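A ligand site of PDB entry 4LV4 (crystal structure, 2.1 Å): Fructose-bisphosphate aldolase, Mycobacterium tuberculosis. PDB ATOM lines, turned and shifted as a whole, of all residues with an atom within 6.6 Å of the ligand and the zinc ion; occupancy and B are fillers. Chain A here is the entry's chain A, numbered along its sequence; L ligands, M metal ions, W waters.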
ATOM      1  N   GLN A  51      -1.453 -25.344 -23.932  1.00  0.00           N
ATOM      2  CA  GLN A  51      -1.155 -26.716 -23.538  1.00  0.00           C
ATOM      3  C   GLN A  51      -2.107 -27.239 -22.480  1.00  0.00           C
ATOM      4  O   GLN A  51      -2.586 -26.489 -21.620  1.00  0.00           O
ATOM      5  CB  GLN A  51       0.320 -26.893 -23.125  1.00  0.00           C
ATOM      6  CG  GLN A  51       0.792 -26.011 -21.958  1.00  0.00           C
ATOM      7  CD  GLN A  51       2.244 -26.294 -21.626  1.00  0.00           C
ATOM      8  OE1 GLN A  51       3.088 -26.444 -22.510  1.00  0.00           O
ATOM      9  NE2 GLN A  51       2.546 -26.374 -20.332  1.00  0.00           N
ATOM     10  N   ASP A  95       1.154 -31.385 -22.069  1.00  0.00           N
ATOM     11  CA  ASP A  95       2.252 -31.214 -21.131  1.00  0.00           C
ATOM     12  C   ASP A  95       2.591 -32.573 -20.530  1.00  0.00           C
ATOM     13  O   ASP A  95       1.946 -33.568 -20.874  1.00  0.00           O
ATOM     14  CB  ASP A  95       1.804 -30.210 -20.040  1.00  0.00           C
ATOM     15  CG  ASP A  95       2.962 -29.612 -19.290  1.00  0.00           C
ATOM     16  OD1 ASP A  95       4.114 -29.810 -19.709  1.00  0.00           O
ATOM     17  OD2 ASP A  95       2.709 -28.900 -18.285  1.00  0.00           O
ATOM     18  N   HIS A  96       3.598 -32.589 -19.647  1.00  0.00           N
ATOM     19  CA  HIS A  96       4.096 -33.791 -18.931  1.00  0.00           C
ATOM     20  C   HIS A  96       3.274 -35.065 -19.039  1.00  0.00           C
ATOM     21  O   HIS A  96       2.226 -35.199 -18.421  1.00  0.00           O
ATOM     22  CB  HIS A  96       4.243 -33.486 -17.439  1.00  0.00           C
ATOM     23  CG  HIS A  96       5.331 -32.514 -17.110  1.00  0.00           C
ATOM     24  ND1 HIS A  96       6.640 -32.895 -16.900  1.00  0.00           N
ATOM     25  CD2 HIS A  96       5.292 -31.175 -16.904  1.00  0.00           C
ATOM     26  CE1 HIS A  96       7.364 -31.827 -16.602  1.00  0.00           C
ATOM     27  NE2 HIS A  96       6.574 -30.772 -16.602  1.00  0.00           N
ATOM     28  N   MET A 129       4.368 -33.585 -25.201  1.00  0.00           N
ATOM     29  CA  MET A 129       5.513 -33.804 -24.326  1.00  0.00           C
ATOM     30  C   MET A 129       5.546 -35.218 -23.792  1.00  0.00           C
ATOM     31  O   MET A 129       4.561 -35.731 -23.253  1.00  0.00           O
ATOM     32  CB  MET A 129       5.543 -32.833 -23.154  1.00  0.00           C
ATOM     33  CG  MET A 129       6.805 -32.997 -22.316  1.00  0.00           C
ATOM     34  SD  MET A 129       6.737 -32.195 -20.694  1.00  0.00           S
ATOM     35  CE  MET A 129       8.475 -32.180 -20.260  1.00  0.00           C
ATOM     36  N   ASP A 131       7.554 -37.053 -20.964  1.00  0.00           N
ATOM     37  CA  ASP A 131       8.384 -36.755 -19.803  1.00  0.00           C
ATOM     38  C   ASP A 131       8.931 -38.062 -19.258  1.00  0.00           C
ATOM     39  O   ASP A 131       8.253 -38.764 -18.508  1.00  0.00           O
ATOM     40  CB  ASP A 131       7.573 -36.030 -18.725  1.00  0.00           C
ATOM     41  CG  ASP A 131       8.389 -35.752 -17.454  1.00  0.00           C
ATOM     42  OD1 ASP A 131       9.601 -36.021 -17.446  1.00  0.00           O
ATOM     43  OD2 ASP A 131       7.822 -35.265 -16.454  1.00  0.00           O
ATOM     44  N   SER A 133      11.742 -38.252 -17.478  1.00  0.00           N
ATOM     45  CA  SER A 133      12.702 -37.912 -16.436  1.00  0.00           C
ATOM     46  C   SER A 133      12.750 -38.920 -15.288  1.00  0.00           C
ATOM     47  O   SER A 133      13.741 -38.988 -14.569  1.00  0.00           O
ATOM     48  CB  SER A 133      12.434 -36.502 -15.889  1.00  0.00           C
ATOM     49  OG  SER A 133      11.156 -36.419 -15.292  1.00  0.00           O
ATOM     50  N   GLU A 159       8.227 -32.858 -27.484  1.00  0.00           N
ATOM     51  CA  GLU A 159       8.986 -32.259 -26.396  1.00  0.00           C
ATOM     52  C   GLU A 159       9.404 -33.385 -25.474  1.00  0.00           C
ATOM     53  O   GLU A 159       8.633 -34.303 -25.210  1.00  0.00           O
ATOM     54  CB  GLU A 159       8.172 -31.205 -25.637  1.00  0.00           C
ATOM     55  CG  GLU A 159       8.916 -30.574 -24.430  1.00  0.00           C
ATOM     56  CD  GLU A 159       8.076 -29.541 -23.672  1.00  0.00           C
ATOM     57  OE1 GLU A 159       7.303 -28.789 -24.314  1.00  0.00           O
ATOM     58  OE2 GLU A 159       8.206 -29.439 -22.437  1.00  0.00           O
ATOM     59  N   GLU A 161      11.959 -34.521 -21.800  1.00  0.00           N
ATOM     60  CA  GLU A 161      12.673 -33.999 -20.652  1.00  0.00           C
ATOM     61  C   GLU A 161      13.767 -34.960 -20.247  1.00  0.00           C
ATOM     62  O   GLU A 161      13.505 -36.126 -19.953  1.00  0.00           O
ATOM     63  CB  GLU A 161      11.747 -33.753 -19.450  1.00  0.00           C
ATOM     64  CG  GLU A 161      12.524 -33.308 -18.217  1.00  0.00           C
ATOM     65  CD  GLU A 161      11.621 -32.743 -17.139  1.00  0.00           C
ATOM     66  OE1 GLU A 161      10.941 -31.745 -17.399  1.00  0.00           O
ATOM     67  OE2 GLU A 161      11.606 -33.304 -16.013  1.00  0.00           O
ATOM     68  N   VAL A 164      17.692 -35.756 -14.453  1.00  0.00           N
ATOM     69  CA  VAL A 164      17.072 -36.196 -13.218  1.00  0.00           C
ATOM     70  C   VAL A 164      16.435 -35.025 -12.459  1.00  0.00           C
ATOM     71  O   VAL A 164      17.011 -33.933 -12.387  1.00  0.00           O
ATOM     72  CB  VAL A 164      18.086 -36.919 -12.330  1.00  0.00           C
ATOM     73  CG1 VAL A 164      18.403 -38.292 -12.906  1.00  0.00           C
ATOM     74  CG2 VAL A 164      19.357 -36.098 -12.214  1.00  0.00           C
ATOM     75  N   VAL A 165      15.248 -35.250 -11.909  1.00  0.00           N
ATOM     76  CA  VAL A 165      14.550 -34.234 -11.140  1.00  0.00           C
ATOM     77  C   VAL A 165      14.941 -34.297  -9.663  1.00  0.00           C
ATOM     78  O   VAL A 165      14.777 -35.318  -9.004  1.00  0.00           O
ATOM     79  CB  VAL A 165      13.020 -34.355 -11.295  1.00  0.00           C
ATOM     80  CG1 VAL A 165      12.303 -33.337 -10.416  1.00  0.00           C
ATOM     81  CG2 VAL A 165      12.630 -34.176 -12.752  1.00  0.00           C
ATOM     82  N   GLY A 166      15.471 -33.185  -9.145  1.00  0.00           N
ATOM     83  CA  GLY A 166      15.873 -33.132  -7.747  1.00  0.00           C
ATOM     84  C   GLY A 166      15.463 -31.833  -7.069  1.00  0.00           C
ATOM     85  O   GLY A 166      15.775 -30.743  -7.548  1.00  0.00           O
ATOM     86  N   GLU A 178      11.863 -27.597  -7.050  1.00  0.00           N
ATOM     87  CA  GLU A 178      12.524 -28.684  -7.773  1.00  0.00           C
ATOM     88  C   GLU A 178      13.246 -28.169  -9.021  1.00  0.00           C
ATOM     89  O   GLU A 178      12.839 -27.171  -9.623  1.00  0.00           O
ATOM     90  CB  GLU A 178      11.523 -29.774  -8.165  1.00  0.00           C
ATOM     91  CG  GLU A 178      10.839 -30.458  -6.978  1.00  0.00           C
ATOM     92  CD  GLU A 178      11.795 -31.306  -6.163  1.00  0.00           C
ATOM     93  OE1 GLU A 178      12.459 -32.191  -6.740  1.00  0.00           O
ATOM     94  OE2 GLU A 178      11.873 -31.093  -4.927  1.00  0.00           O
ATOM     95  N   LYS A 179      14.320 -28.863  -9.396  1.00  0.00           N
ATOM     96  CA  LYS A 179      15.142 -28.471 -10.537  1.00  0.00           C
ATOM     97  C   LYS A 179      15.596 -29.683 -11.347  1.00  0.00           C
ATOM     98  O   LYS A 179      15.649 -30.803 -10.846  1.00  0.00           O
ATOM     99  CB  LYS A 179      16.350 -27.655 -10.084  1.00  0.00           C
ATOM    100  CG  LYS A 179      16.133 -26.143 -10.089  1.00  0.00           C
ATOM    101  CD  LYS A 179      16.440 -25.572 -11.461  1.00  0.00           C
ATOM    102  CE  LYS A 179      17.774 -26.099 -11.981  1.00  0.00           C
ATOM    103  NZ  LYS A 179      18.206 -25.445 -13.247  1.00  0.00           N
ATOM    104  N   LEU A 180      15.943 -29.441 -12.610  1.00  0.00           N
ATOM    105  CA  LEU A 180      16.330 -30.497 -13.532  1.00  0.00           C
ATOM    106  C   LEU A 180      17.830 -30.460 -13.827  1.00  0.00           C
ATOM    107  O   LEU A 180      18.311 -29.530 -14.481  1.00  0.00           O
ATOM    108  CB  LEU A 180      15.569 -30.352 -14.855  1.00  0.00           C
ATOM    109  CG  LEU A 180      15.846 -31.384 -15.958  1.00  0.00           C
ATOM    110  CD1 LEU A 180      15.342 -32.765 -15.561  1.00  0.00           C
ATOM    111  CD2 LEU A 180      15.221 -30.932 -17.274  1.00  0.00           C
ATOM    112  N   ALA A 205      13.337 -30.036 -22.526  1.00  0.00           N
ATOM    113  CA  ALA A 205      13.010 -29.298 -21.301  1.00  0.00           C
ATOM    114  C   ALA A 205      14.241 -28.880 -20.517  1.00  0.00           C
ATOM    115  O   ALA A 205      15.288 -29.526 -20.570  1.00  0.00           O
ATOM    116  CB  ALA A 205      12.069 -30.089 -20.411  1.00  0.00           C
ATOM    117  N   ALA A 206      14.086 -27.800 -19.771  1.00  0.00           N
ATOM    118  CA  ALA A 206      15.167 -27.275 -18.953  1.00  0.00           C
ATOM    119  C   ALA A 206      14.559 -26.407 -17.864  1.00  0.00           C
ATOM    120  O   ALA A 206      13.425 -25.906 -17.997  1.00  0.00           O
ATOM    121  CB  ALA A 206      16.129 -26.475 -19.814  1.00  0.00           C
ATOM    122  N   THR A 207      15.308 -26.231 -16.778  1.00  0.00           N
ATOM    123  CA  THR A 207      14.938 -25.322 -15.694  1.00  0.00           C
ATOM    124  C   THR A 207      16.058 -24.317 -15.459  1.00  0.00           C
ATOM    125  O   THR A 207      17.107 -24.364 -16.133  1.00  0.00           O
ATOM    126  CB  THR A 207      14.622 -26.070 -14.369  1.00  0.00           C
ATOM    127  OG1 THR A 207      15.704 -26.941 -14.031  1.00  0.00           O
ATOM    128  CG2 THR A 207      13.349 -26.892 -14.507  1.00  0.00           C
ATOM    129  N   HIS A 252      10.838 -24.809 -18.091  1.00  0.00           N
ATOM    130  CA  HIS A 252       9.864 -25.281 -17.104  1.00  0.00           C
ATOM    131  C   HIS A 252      10.134 -24.671 -15.716  1.00  0.00           C
ATOM    132  O   HIS A 252      11.280 -24.361 -15.371  1.00  0.00           O
ATOM    133  CB  HIS A 252       9.931 -26.804 -16.973  1.00  0.00           C
ATOM    134  CG  HIS A 252       9.361 -27.555 -18.139  1.00  0.00           C
ATOM    135  ND1 HIS A 252       8.328 -28.449 -18.003  1.00  0.00           N
ATOM    136  CD2 HIS A 252       9.691 -27.544 -19.456  1.00  0.00           C
ATOM    137  CE1 HIS A 252       8.023 -28.957 -19.186  1.00  0.00           C
ATOM    138  NE2 HIS A 252       8.847 -28.430 -20.081  1.00  0.00           N
ATOM    139  N   GLY A 253       9.083 -24.530 -14.921  1.00  0.00           N
ATOM    140  CA  GLY A 253       9.220 -24.081 -13.534  1.00  0.00           C
ATOM    141  C   GLY A 253       9.653 -22.631 -13.397  1.00  0.00           C
ATOM    142  O   GLY A 253      10.366 -22.273 -12.458  1.00  0.00           O
ATOM    143  N   GLY A 254       9.207 -21.777 -14.308  1.00  0.00           N
ATOM    144  CA  GLY A 254       9.693 -20.402 -14.333  1.00  0.00           C
ATOM    145  C   GLY A 254       8.741 -19.373 -13.743  1.00  0.00           C
ATOM    146  O   GLY A 254       8.907 -18.175 -13.976  1.00  0.00           O
ATOM    147  N   SER A 255       7.751 -19.841 -12.969  1.00  0.00           N
ATOM    148  CA  SER A 255       6.751 -18.946 -12.380  1.00  0.00           C
ATOM    149  C   SER A 255       7.376 -17.760 -11.685  1.00  0.00           C
ATOM    150  O   SER A 255       8.339 -17.900 -10.930  1.00  0.00           O
ATOM    151  CB  SER A 255       5.878 -19.706 -11.382  1.00  0.00           C
ATOM    152  OG  SER A 255       5.053 -20.646 -12.057  1.00  0.00           O
ATOM    153  N   ASN A 274       6.873 -22.419 -20.211  1.00  0.00           N
ATOM    154  CA  ASN A 274       5.608 -22.911 -19.698  1.00  0.00           C
ATOM    155  C   ASN A 274       5.078 -22.018 -18.587  1.00  0.00           C
ATOM    156  O   ASN A 274       5.826 -21.617 -17.701  1.00  0.00           O
ATOM    157  CB  ASN A 274       5.740 -24.367 -19.220  1.00  0.00           C
ATOM    158  CG  ASN A 274       5.999 -25.356 -20.366  1.00  0.00           C
ATOM    159  OD1 ASN A 274       6.255 -24.961 -21.518  1.00  0.00           O
ATOM    160  ND2 ASN A 274       5.928 -26.642 -20.066  1.00  0.00           N
ATOM    161  N   ASP A 276       1.696 -21.524 -15.885  1.00  0.00           N
ATOM    162  CA  ASP A 276       0.423 -22.009 -15.330  1.00  0.00           C
ATOM    163  C   ASP A 276       0.068 -21.228 -14.071  1.00  0.00           C
ATOM    164  O   ASP A 276      -0.937 -20.515 -14.028  1.00  0.00           O
ATOM    165  CB  ASP A 276       0.496 -23.524 -15.047  1.00  0.00           C
ATOM    166  CG  ASP A 276      -0.835 -24.120 -14.629  1.00  0.00           C
ATOM    167  OD1 ASP A 276      -1.916 -23.546 -14.931  1.00  0.00           O
ATOM    168  OD2 ASP A 276      -0.820 -25.197 -13.994  1.00  0.00           O
ATOM    169  N   THR A 277       0.920 -21.344 -13.051  1.00  0.00           N
ATOM    170  CA  THR A 277       0.710 -20.668 -11.771  1.00  0.00           C
ATOM    171  C   THR A 277       0.329 -19.197 -11.937  1.00  0.00           C
ATOM    172  O   THR A 277      -0.638 -18.719 -11.341  1.00  0.00           O
ATOM    173  CB  THR A 277       1.968 -20.763 -10.889  1.00  0.00           C
ATOM    174  OG1 THR A 277       2.215 -22.143 -10.592  1.00  0.00           O
ATOM    175  CG2 THR A 277       1.779 -19.998  -9.585  1.00  0.00           C
HETATM  176  O1  LIG L   1       5.494 -26.717 -13.986  1.00  0.00           O
HETATM  177  C1  LIG L   1       6.315 -27.528 -14.475  1.00  0.00           C
HETATM  178  O2  LIG L   1       6.148 -28.073 -15.636  1.00  0.00           O
HETATM  179  C2  LIG L   1       7.547 -27.838 -13.699  1.00  0.00           C
HETATM  180  N1  LIG L   1       8.384 -28.651 -14.320  1.00  0.00           N
HETATM  181  C3  LIG L   1       9.548 -29.054 -13.800  1.00  0.00           C
HETATM  182  C4  LIG L   1       9.941 -28.616 -12.559  1.00  0.00           C
HETATM  183  C5  LIG L   1      11.180 -29.067 -12.048  1.00  0.00           C
HETATM  184  C6  LIG L   1      11.973 -29.941 -12.829  1.00  0.00           C
HETATM  185  C7  LIG L   1      11.533 -30.372 -14.096  1.00  0.00           C
HETATM  186  C8  LIG L   1      10.316 -29.916 -14.588  1.00  0.00           C
HETATM  187  O3  LIG L   1       9.763 -30.253 -15.803  1.00  0.00           O
HETATM  188  C9  LIG L   1       9.074 -27.729 -11.841  1.00  0.00           C
HETATM  189  C10 LIG L   1       7.852 -27.336 -12.435  1.00  0.00           C
HETATM  190 ZN    ZN M   1       7.804 -29.236 -16.149  1.00  0.00          ZN
HETATM  191  O   HOH W   1       4.462 -27.275 -17.443  1.00  0.00           O
HETATM  192  O   HOH W   2       6.789 -24.767 -15.801  1.00  0.00           O
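O of Glu 178 touches C5 of the ligand, 3.5 Å away.
Lys 179 touches the ligand (C to C6, 3.9 Å).
Thr 207 touches the ligand (CG2 to C6, 3.7 Å).
Gly 253 touches the ligand (CA to C10, 3.7 Å).
Of the 24 residues printed, 7 come within 4 Å of the ligand.
The nearest printed residue that does not touch the ligand is Leu 180 (4.01 Å).
The side-chain sulfur (SD) of Met 129 sits at hydrogen-bond distance from the backbone NH (N) of His 96 (3.3 Å).
NE2 of His 252 sits close to ND2 of Asn 274 (3.4 Å).
O of Ala 206 is in hydrogen-bond range of N of His 252 (2.8 Å).
The side-chain carboxylate of Glu 159 sits at hydrogen-bond distance from a ring nitrogen (NE2) of His 252 (2.6 Å).
OG of Ser 133 is in hydrogen-bond range of OE2 of Glu 161.
The side-chain amino group of Lys 179 lies close to the side-chain hydroxyl of Thr 207 (3.0 Å).
The backbone NH of Leu 180 lies within hydrogen-bond range of the side-chain hydroxyl of Thr 207 (2.9 Å).
O of Lys 179 lies within hydrogen-bond range of N of Gly 166 (2.9 Å).
The nearest printed residue that does not touch the zinc ion is Glu 161 (4.2 Å).
The side-chain carboxylate (OE1) of Glu 161 lies close to an oxygen (O3) of the ligand, at 2.5 Å.
Water W1 bridges the side-chain carboxylate (OD2) of Asp 95 and the side-chain amide nitrogen (ND2) of Asn 274.
Water W2 lies within hydrogen-bond range of the backbone NH of Gly 253 (2.5 Å) and an oxygen (O1) of the ligand (3.0 Å).
The zinc ion is bound by N1 of the ligand (2.0 Å), NE2 of His 96 (2.0 Å), ND1 of His 252 (2.1 Å), O2 of the ligand (2.1 Å) and O3 of the ligand (2.2 Å).
The zinc ion has five donor atoms within binding distance.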
